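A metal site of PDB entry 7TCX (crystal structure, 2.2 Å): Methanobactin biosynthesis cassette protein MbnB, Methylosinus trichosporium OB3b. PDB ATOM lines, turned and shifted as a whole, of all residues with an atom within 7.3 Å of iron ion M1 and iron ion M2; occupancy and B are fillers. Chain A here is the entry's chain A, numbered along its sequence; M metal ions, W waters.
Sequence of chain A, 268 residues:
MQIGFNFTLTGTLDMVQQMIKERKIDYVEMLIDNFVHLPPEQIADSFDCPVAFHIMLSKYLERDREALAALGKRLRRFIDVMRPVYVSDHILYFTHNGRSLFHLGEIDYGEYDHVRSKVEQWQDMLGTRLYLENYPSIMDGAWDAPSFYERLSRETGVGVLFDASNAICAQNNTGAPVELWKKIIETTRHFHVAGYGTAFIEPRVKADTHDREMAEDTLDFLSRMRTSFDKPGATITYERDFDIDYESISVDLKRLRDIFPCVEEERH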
ATOM      1  N   GLU A  29     -15.688 -23.171  20.176  1.00  0.00           N
ATOM      2  CA  GLU A  29     -15.808 -22.258  19.048  1.00  0.00           C
ATOM      3  C   GLU A  29     -17.264 -22.275  18.571  1.00  0.00           C
ATOM      4  O   GLU A  29     -17.736 -23.289  18.046  1.00  0.00           O
ATOM      5  CB  GLU A  29     -14.851 -22.635  17.930  1.00  0.00           C
ATOM      6  CG  GLU A  29     -14.660 -21.560  16.870  1.00  0.00           C
ATOM      7  CD  GLU A  29     -13.877 -22.063  15.673  1.00  0.00           C
ATOM      8  OE1 GLU A  29     -12.627 -22.055  15.731  1.00  0.00           O
ATOM      9  OE2 GLU A  29     -14.520 -22.484  14.675  1.00  0.00           O
ATOM     10  N   LEU A  31     -20.245 -21.430  16.111  1.00  0.00           N
ATOM     11  CA  LEU A  31     -20.709 -20.970  14.801  1.00  0.00           C
ATOM     12  C   LEU A  31     -21.756 -19.890  15.058  1.00  0.00           C
ATOM     13  O   LEU A  31     -22.968 -20.101  14.954  1.00  0.00           O
ATOM     14  CB  LEU A  31     -21.266 -22.130  13.969  1.00  0.00           C
ATOM     15  CG  LEU A  31     -21.134 -21.972  12.462  1.00  0.00           C
ATOM     16  CD1 LEU A  31     -19.653 -22.048  12.038  1.00  0.00           C
ATOM     17  CD2 LEU A  31     -21.953 -23.025  11.703  1.00  0.00           C
ATOM     18  N   HIS A  54     -16.894 -18.181  15.060  1.00  0.00           N
ATOM     19  CA  HIS A  54     -16.728 -18.544  13.653  1.00  0.00           C
ATOM     20  C   HIS A  54     -18.010 -18.144  12.938  1.00  0.00           C
ATOM     21  O   HIS A  54     -19.097 -18.538  13.352  1.00  0.00           O
ATOM     22  CB  HIS A  54     -16.464 -20.047  13.526  1.00  0.00           C
ATOM     23  CG  HIS A  54     -15.776 -20.449  12.257  1.00  0.00           C
ATOM     24  ND1 HIS A  54     -14.652 -19.819  11.766  1.00  0.00           N
ATOM     25  CD2 HIS A  54     -16.030 -21.479  11.410  1.00  0.00           C
ATOM     26  CE1 HIS A  54     -14.270 -20.414  10.653  1.00  0.00           C
ATOM     27  NE2 HIS A  54     -15.086 -21.429  10.424  1.00  0.00           N
ATOM     28  N   ILE A  55     -17.893 -17.327  11.898  1.00  0.00           N
ATOM     29  CA  ILE A  55     -19.040 -16.786  11.166  1.00  0.00           C
ATOM     30  C   ILE A  55     -19.113 -17.478   9.805  1.00  0.00           C
ATOM     31  O   ILE A  55     -18.177 -17.378   9.006  1.00  0.00           O
ATOM     32  CB  ILE A  55     -18.920 -15.267  10.984  1.00  0.00           C
ATOM     33  CG1 ILE A  55     -18.813 -14.537  12.342  1.00  0.00           C
ATOM     34  CG2 ILE A  55     -20.075 -14.746  10.132  1.00  0.00           C
ATOM     35  CD1 ILE A  55     -17.998 -13.243  12.273  1.00  0.00           C
ATOM     36  N   MET A  56     -20.234 -18.158   9.541  1.00  0.00           N
ATOM     37  CA  MET A  56     -20.374 -18.946   8.316  1.00  0.00           C
ATOM     38  C   MET A  56     -21.087 -18.187   7.202  1.00  0.00           C
ATOM     39  O   MET A  56     -20.612 -18.167   6.054  1.00  0.00           O
ATOM     40  CB  MET A  56     -21.129 -20.241   8.603  1.00  0.00           C
ATOM     41  CG  MET A  56     -21.314 -21.154   7.367  1.00  0.00           C
ATOM     42  SD  MET A  56     -19.769 -21.562   6.487  1.00  0.00           S
ATOM     43  CE  MET A  56     -19.220 -22.886   7.548  1.00  0.00           C
ATOM     44  N   SER A  88     -13.681 -15.019  13.567  1.00  0.00           N
ATOM     45  CA  SER A  88     -13.225 -15.544  12.275  1.00  0.00           C
ATOM     46  C   SER A  88     -14.381 -15.687  11.293  1.00  0.00           C
ATOM     47  O   SER A  88     -15.550 -15.793  11.649  1.00  0.00           O
ATOM     48  CB  SER A  88     -12.496 -16.888  12.431  1.00  0.00           C
ATOM     49  OG  SER A  88     -13.276 -17.823  13.142  1.00  0.00           O
ATOM     50  N   ASP A  89     -14.021 -15.668  10.007  1.00  0.00           N
ATOM     51  CA  ASP A  89     -14.980 -15.769   8.922  1.00  0.00           C
ATOM     52  C   ASP A  89     -14.262 -16.416   7.739  1.00  0.00           C
ATOM     53  O   ASP A  89     -13.165 -16.970   7.890  1.00  0.00           O
ATOM     54  CB  ASP A  89     -15.589 -14.384   8.620  1.00  0.00           C
ATOM     55  CG  ASP A  89     -16.939 -14.460   7.886  1.00  0.00           C
ATOM     56  OD1 ASP A  89     -17.157 -15.331   6.982  1.00  0.00           O
ATOM     57  OD2 ASP A  89     -17.802 -13.618   8.212  1.00  0.00           O
ATOM     58  N   HIS A  90     -14.866 -16.343   6.554  1.00  0.00           N
ATOM     59  CA  HIS A  90     -14.450 -17.159   5.427  1.00  0.00           C
ATOM     60  C   HIS A  90     -14.195 -16.306   4.196  1.00  0.00           C
ATOM     61  O   HIS A  90     -14.593 -15.140   4.128  1.00  0.00           O
ATOM     62  CB  HIS A  90     -15.510 -18.207   5.083  1.00  0.00           C
ATOM     63  CG  HIS A  90     -15.716 -19.234   6.138  1.00  0.00           C
ATOM     64  ND1 HIS A  90     -16.536 -19.015   7.231  1.00  0.00           N
ATOM     65  CD2 HIS A  90     -15.226 -20.487   6.276  1.00  0.00           C
ATOM     66  CE1 HIS A  90     -16.531 -20.098   7.991  1.00  0.00           C
ATOM     67  NE2 HIS A  90     -15.736 -21.005   7.438  1.00  0.00           N
ATOM     68  N   LEU A  92     -15.462 -17.166   0.709  1.00  0.00           N
ATOM     69  CA  LEU A  92     -16.258 -18.135  -0.018  1.00  0.00           C
ATOM     70  C   LEU A  92     -17.110 -17.458  -1.086  1.00  0.00           C
ATOM     71  O   LEU A  92     -17.500 -16.290  -0.961  1.00  0.00           O
ATOM     72  CB  LEU A  92     -17.188 -18.932   0.917  1.00  0.00           C
ATOM     73  CG  LEU A  92     -16.477 -19.867   1.870  1.00  0.00           C
ATOM     74  CD1 LEU A  92     -17.400 -20.185   3.002  1.00  0.00           C
ATOM     75  CD2 LEU A  92     -16.060 -21.137   1.136  1.00  0.00           C
ATOM     76  N   GLU A 133     -10.321 -17.792   7.024  1.00  0.00           N
ATOM     77  CA  GLU A 133      -9.926 -19.186   6.913  1.00  0.00           C
ATOM     78  C   GLU A 133      -9.595 -19.544   5.464  1.00  0.00           C
ATOM     79  O   GLU A 133     -10.196 -19.022   4.526  1.00  0.00           O
ATOM     80  CB  GLU A 133     -11.052 -20.068   7.444  1.00  0.00           C
ATOM     81  CG  GLU A 133     -10.912 -21.550   7.130  1.00  0.00           C
ATOM     82  CD  GLU A 133     -11.878 -22.405   7.885  1.00  0.00           C
ATOM     83  OE1 GLU A 133     -13.006 -21.933   8.161  1.00  0.00           O
ATOM     84  OE2 GLU A 133     -11.546 -23.548   8.197  1.00  0.00           O
ATOM     85  N   ASN A 134      -8.610 -20.447   5.289  1.00  0.00           N
ATOM     86  CA  ASN A 134      -8.288 -20.992   3.959  1.00  0.00           C
ATOM     87  C   ASN A 134      -9.321 -22.037   3.512  1.00  0.00           C
ATOM     88  O   ASN A 134      -9.913 -22.736   4.320  1.00  0.00           O
ATOM     89  CB  ASN A 134      -6.905 -21.654   3.945  1.00  0.00           C
ATOM     90  CG  ASN A 134      -6.741 -22.672   5.069  1.00  0.00           C
ATOM     91  OD1 ASN A 134      -7.004 -22.368   6.259  1.00  0.00           O
ATOM     92  ND2 ASN A 134      -6.282 -23.870   4.706  1.00  0.00           N
ATOM     93  N   LEU A 161      -6.976 -17.758   9.956  1.00  0.00           N
ATOM     94  CA  LEU A 161      -7.323 -18.964  10.695  1.00  0.00           C
ATOM     95  C   LEU A 161      -6.897 -20.129   9.809  1.00  0.00           C
ATOM     96  O   LEU A 161      -7.509 -20.369   8.764  1.00  0.00           O
ATOM     97  CB  LEU A 161      -8.805 -19.021  11.012  1.00  0.00           C
ATOM     98  CG  LEU A 161      -9.339 -20.251  11.758  1.00  0.00           C
ATOM     99  CD1 LEU A 161      -8.828 -20.324  13.184  1.00  0.00           C
ATOM    100  CD2 LEU A 161     -10.853 -20.240  11.753  1.00  0.00           C
ATOM    101  N   PHE A 162      -5.814 -20.802  10.176  1.00  0.00           N
ATOM    102  CA  PHE A 162      -5.246 -21.796   9.282  1.00  0.00           C
ATOM    103  C   PHE A 162      -5.896 -23.145   9.602  1.00  0.00           C
ATOM    104  O   PHE A 162      -5.745 -23.681  10.713  1.00  0.00           O
ATOM    105  CB  PHE A 162      -3.731 -21.853   9.380  1.00  0.00           C
ATOM    106  CG  PHE A 162      -3.145 -22.878   8.461  1.00  0.00           C
ATOM    107  CD1 PHE A 162      -3.180 -22.701   7.080  1.00  0.00           C
ATOM    108  CD2 PHE A 162      -2.639 -24.069   8.947  1.00  0.00           C
ATOM    109  CE1 PHE A 162      -2.714 -23.655   6.214  1.00  0.00           C
ATOM    110  CE2 PHE A 162      -2.144 -25.029   8.088  1.00  0.00           C
ATOM    111  CZ  PHE A 162      -2.170 -24.814   6.721  1.00  0.00           C
ATOM    112  N   ASP A 163      -6.636 -23.674   8.642  1.00  0.00           N
ATOM    113  CA  ASP A 163      -7.255 -24.977   8.789  1.00  0.00           C
ATOM    114  C   ASP A 163      -6.313 -25.998   8.155  1.00  0.00           C
ATOM    115  O   ASP A 163      -6.170 -26.058   6.923  1.00  0.00           O
ATOM    116  CB  ASP A 163      -8.632 -24.995   8.141  1.00  0.00           C
ATOM    117  CG  ASP A 163      -9.373 -26.302   8.377  1.00  0.00           C
ATOM    118  OD1 ASP A 163      -8.773 -27.369   8.150  1.00  0.00           O
ATOM    119  OD2 ASP A 163     -10.541 -26.263   8.822  1.00  0.00           O
ATOM    120  N   ALA A 164      -5.667 -26.813   9.005  1.00  0.00           N
ATOM    121  CA  ALA A 164      -4.644 -27.741   8.526  1.00  0.00           C
ATOM    122  C   ALA A 164      -5.233 -28.820   7.609  1.00  0.00           C
ATOM    123  O   ALA A 164      -4.600 -29.249   6.638  1.00  0.00           O
ATOM    124  CB  ALA A 164      -3.949 -28.392   9.720  1.00  0.00           C
ATOM    125  N   SER A 165      -6.444 -29.291   7.912  1.00  0.00           N
ATOM    126  CA  SER A 165      -6.940 -30.364   7.061  1.00  0.00           C
ATOM    127  C   SER A 165      -7.474 -29.825   5.734  1.00  0.00           C
ATOM    128  O   SER A 165      -7.387 -30.533   4.723  1.00  0.00           O
ATOM    129  CB  SER A 165      -7.993 -31.203   7.811  1.00  0.00           C
ATOM    130  OG  SER A 165      -9.068 -30.463   8.361  1.00  0.00           O
ATOM    131  N   ASN A 166      -7.999 -28.592   5.690  1.00  0.00           N
ATOM    132  CA  ASN A 166      -8.349 -27.995   4.403  1.00  0.00           C
ATOM    133  C   ASN A 166      -7.120 -27.897   3.503  1.00  0.00           C
ATOM    134  O   ASN A 166      -7.219 -28.089   2.289  1.00  0.00           O
ATOM    135  CB  ASN A 166      -8.941 -26.608   4.561  1.00  0.00           C
ATOM    136  CG  ASN A 166     -10.252 -26.619   5.262  1.00  0.00           C
ATOM    137  OD1 ASN A 166     -10.695 -27.671   5.707  1.00  0.00           O
ATOM    138  ND2 ASN A 166     -10.873 -25.447   5.419  1.00  0.00           N
ATOM    139  N   PHE A 191      -5.962 -22.113  14.803  1.00  0.00           N
ATOM    140  CA  PHE A 191      -5.952 -23.203  13.850  1.00  0.00           C
ATOM    141  C   PHE A 191      -7.263 -23.989  13.881  1.00  0.00           C
ATOM    142  O   PHE A 191      -8.025 -23.931  14.849  1.00  0.00           O
ATOM    143  CB  PHE A 191      -4.776 -24.153  14.110  1.00  0.00           C
ATOM    144  CG  PHE A 191      -3.435 -23.499  13.908  1.00  0.00           C
ATOM    145  CD1 PHE A 191      -2.947 -23.301  12.630  1.00  0.00           C
ATOM    146  CD2 PHE A 191      -2.699 -23.034  14.991  1.00  0.00           C
ATOM    147  CE1 PHE A 191      -1.708 -22.673  12.439  1.00  0.00           C
ATOM    148  CE2 PHE A 191      -1.466 -22.384  14.809  1.00  0.00           C
ATOM    149  CZ  PHE A 191      -0.964 -22.207  13.533  1.00  0.00           C
ATOM    150  N   HIS A 192      -7.501 -24.698  12.778  1.00  0.00           N
ATOM    151  CA  HIS A 192      -8.558 -25.688  12.637  1.00  0.00           C
ATOM    152  C   HIS A 192      -7.961 -27.009  12.176  1.00  0.00           C
ATOM    153  O   HIS A 192      -6.922 -27.058  11.519  1.00  0.00           O
ATOM    154  CB  HIS A 192      -9.580 -25.304  11.573  1.00  0.00           C
ATOM    155  CG  HIS A 192     -10.697 -24.452  12.057  1.00  0.00           C
ATOM    156  ND1 HIS A 192     -11.832 -24.239  11.315  1.00  0.00           N
ATOM    157  CD2 HIS A 192     -10.837 -23.720  13.186  1.00  0.00           C
ATOM    158  CE1 HIS A 192     -12.639 -23.434  11.978  1.00  0.00           C
ATOM    159  NE2 HIS A 192     -12.063 -23.109  13.112  1.00  0.00           N
ATOM    160  N   VAL A 193      -8.681 -28.085  12.492  1.00  0.00           N
ATOM    161  CA  VAL A 193      -8.377 -29.392  11.933  1.00  0.00           C
ATOM    162  C   VAL A 193      -9.633 -30.243  12.049  1.00  0.00           C
ATOM    163  O   VAL A 193     -10.452 -30.038  12.964  1.00  0.00           O
ATOM    164  CB  VAL A 193      -7.158 -30.031  12.649  1.00  0.00           C
ATOM    165  CG1 VAL A 193      -7.529 -30.464  14.056  1.00  0.00           C
ATOM    166  CG2 VAL A 193      -6.656 -31.205  11.843  1.00  0.00           C
ATOM    167  N   ALA A 194      -9.809 -31.166  11.100  1.00  0.00           N
ATOM    168  CA  ALA A 194     -10.965 -32.051  11.060  1.00  0.00           C
ATOM    169  C   ALA A 194     -10.651 -33.252  10.170  1.00  0.00           C
ATOM    170  O   ALA A 194      -9.590 -33.332   9.545  1.00  0.00           O
ATOM    171  CB  ALA A 194     -12.208 -31.324  10.560  1.00  0.00           C
ATOM    172  N   ASP A 208     -14.208 -31.791   2.095  1.00  0.00           N
ATOM    173  CA  ASP A 208     -14.045 -31.236   3.451  1.00  0.00           C
ATOM    174  C   ASP A 208     -15.341 -31.395   4.233  1.00  0.00           C
ATOM    175  O   ASP A 208     -16.146 -30.471   4.371  1.00  0.00           O
ATOM    176  CB  ASP A 208     -13.621 -29.774   3.367  1.00  0.00           C
ATOM    177  CG  ASP A 208     -13.151 -29.224   4.716  1.00  0.00           C
ATOM    178  OD1 ASP A 208     -12.329 -29.892   5.376  1.00  0.00           O
ATOM    179  OD2 ASP A 208     -13.618 -28.116   5.107  1.00  0.00           O
ATOM    180  N   HIS A 210     -15.844 -32.967   7.552  1.00  0.00           N
ATOM    181  CA  HIS A 210     -15.853 -32.865   9.023  1.00  0.00           C
ATOM    182  C   HIS A 210     -16.717 -33.934   9.665  1.00  0.00           C
ATOM    183  O   HIS A 210     -17.457 -33.678  10.606  1.00  0.00           O
ATOM    184  CB  HIS A 210     -16.339 -31.492   9.505  1.00  0.00           C
ATOM    185  CG  HIS A 210     -15.587 -30.353   8.910  1.00  0.00           C
ATOM    186  ND1 HIS A 210     -15.947 -29.045   9.131  1.00  0.00           N
ATOM    187  CD2 HIS A 210     -14.487 -30.321   8.124  1.00  0.00           C
ATOM    188  CE1 HIS A 210     -15.115 -28.250   8.483  1.00  0.00           C
ATOM    189  NE2 HIS A 210     -14.222 -29.003   7.858  1.00  0.00           N
ATOM    190  N   THR A 237      -8.975 -25.725  16.882  1.00  0.00           N
ATOM    191  CA  THR A 237     -10.335 -26.226  16.997  1.00  0.00           C
ATOM    192  C   THR A 237     -10.476 -27.514  16.199  1.00  0.00           C
ATOM    193  O   THR A 237     -10.185 -27.539  15.009  1.00  0.00           O
ATOM    194  CB  THR A 237     -11.341 -25.202  16.484  1.00  0.00           C
ATOM    195  OG1 THR A 237     -11.100 -23.924  17.071  1.00  0.00           O
ATOM    196  CG2 THR A 237     -12.774 -25.659  16.777  1.00  0.00           C
ATOM    197  N   GLU A 239     -13.004 -29.869  14.394  1.00  0.00           N
ATOM    198  CA  GLU A 239     -14.329 -29.692  13.802  1.00  0.00           C
ATOM    199  C   GLU A 239     -14.976 -31.054  13.565  1.00  0.00           C
ATOM    200  O   GLU A 239     -14.361 -31.935  12.957  1.00  0.00           O
ATOM    201  CB  GLU A 239     -14.260 -28.924  12.492  1.00  0.00           C
ATOM    202  CG  GLU A 239     -13.465 -27.642  12.574  1.00  0.00           C
ATOM    203  CD  GLU A 239     -13.571 -26.822  11.306  1.00  0.00           C
ATOM    204  OE1 GLU A 239     -14.583 -26.120  11.101  1.00  0.00           O
ATOM    205  OE2 GLU A 239     -12.620 -26.900  10.498  1.00  0.00           O
ATOM    206  N   ASP A 241     -18.858 -31.975  12.271  1.00  0.00           N
ATOM    207  CA  ASP A 241     -20.165 -31.451  11.913  1.00  0.00           C
ATOM    208  C   ASP A 241     -21.196 -32.538  11.651  1.00  0.00           C
ATOM    209  O   ASP A 241     -22.392 -32.264  11.667  1.00  0.00           O
ATOM    210  CB  ASP A 241     -20.041 -30.541  10.683  1.00  0.00           C
ATOM    211  CG  ASP A 241     -19.210 -29.278  10.966  1.00  0.00           C
ATOM    212  OD1 ASP A 241     -19.263 -28.767  12.105  1.00  0.00           O
ATOM    213  OD2 ASP A 241     -18.500 -28.789  10.069  1.00  0.00           O
HETATM  214 FE    FE M   1     -12.305 -25.193   9.174  1.00  0.00          FE
HETATM  215 FE    FE M   2     -15.006 -22.709   8.511  1.00  0.00          FE
HETATM  216 FE    FE M   3     -12.454 -27.945   6.969  1.00  0.00          FE
HETATM  217  O   HOH W   1     -14.972 -23.968   6.438  1.00  0.00           O
HETATM  218  O   HOH W   2     -14.233 -24.290   9.265  1.00  0.00           O
HETATM  219  O   HOH W   3     -13.370 -25.875   7.092  1.00  0.00           O
HETATM  220  O   HOH W   4     -17.097 -23.673   9.200  1.00  0.00           O
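Iron ion M1 is bound by the side-chain carboxylate (OE2) of Glu 133 (2.1 Å), the side-chain carboxylate (OD2) of Asp 163 (2.1 Å), water W2 (2.1 Å), the side-chain carboxylate (OE2) of Glu 239 (2.2 Å), a ring nitrogen (ND1) of His 192 (2.4 Å) and water W3 (2.4 Å).
Iron ion M2 is bound by water W2 (1.9 Å), a ring nitrogen (NE2) of His 90 (2.1 Å), the side-chain carboxylate (OE1) of Glu 133 (2.2 Å), a ring nitrogen (NE2) of His 54 (2.3 Å), water W4 (2.4 Å) and water W1 (2.4 Å).
Iron ion M2 has six donor atoms within binding distance.
Of the 26 residues printed, 4 come within 4 Å of iron ion M1.
Along chain A the residues within 4 Å of iron ion M1 span positions 133 to 239.
N of Glu 133 sits at hydrogen-bond distance from O of Asp 89 (3.1 Å).
The side-chain amide oxygen (OD1) of Asn 134 sits at hydrogen-bond distance from the backbone NH (N) of Asp 163 (2.7 Å).
N of Ser 165 sits at hydrogen-bond distance from OD1 of Asp 163 (3.0 Å).
O of Ile 55 is in hydrogen-bond range of ND1 of His 90 (2.9 Å).
N of Glu 239 lies within hydrogen-bond range of O of Val 193.
A ring nitrogen (ND1) of His 54 lies within hydrogen-bond range of the side-chain hydroxyl (OG) of Ser 88, at 2.8 Å.
The backbone carbonyl oxygen of Phe 162 lies within hydrogen-bond range of the backbone NH of His 192, at 2.9 Å.
O of His 192 lies within hydrogen-bond range of N of Ala 164 (2.8 Å).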
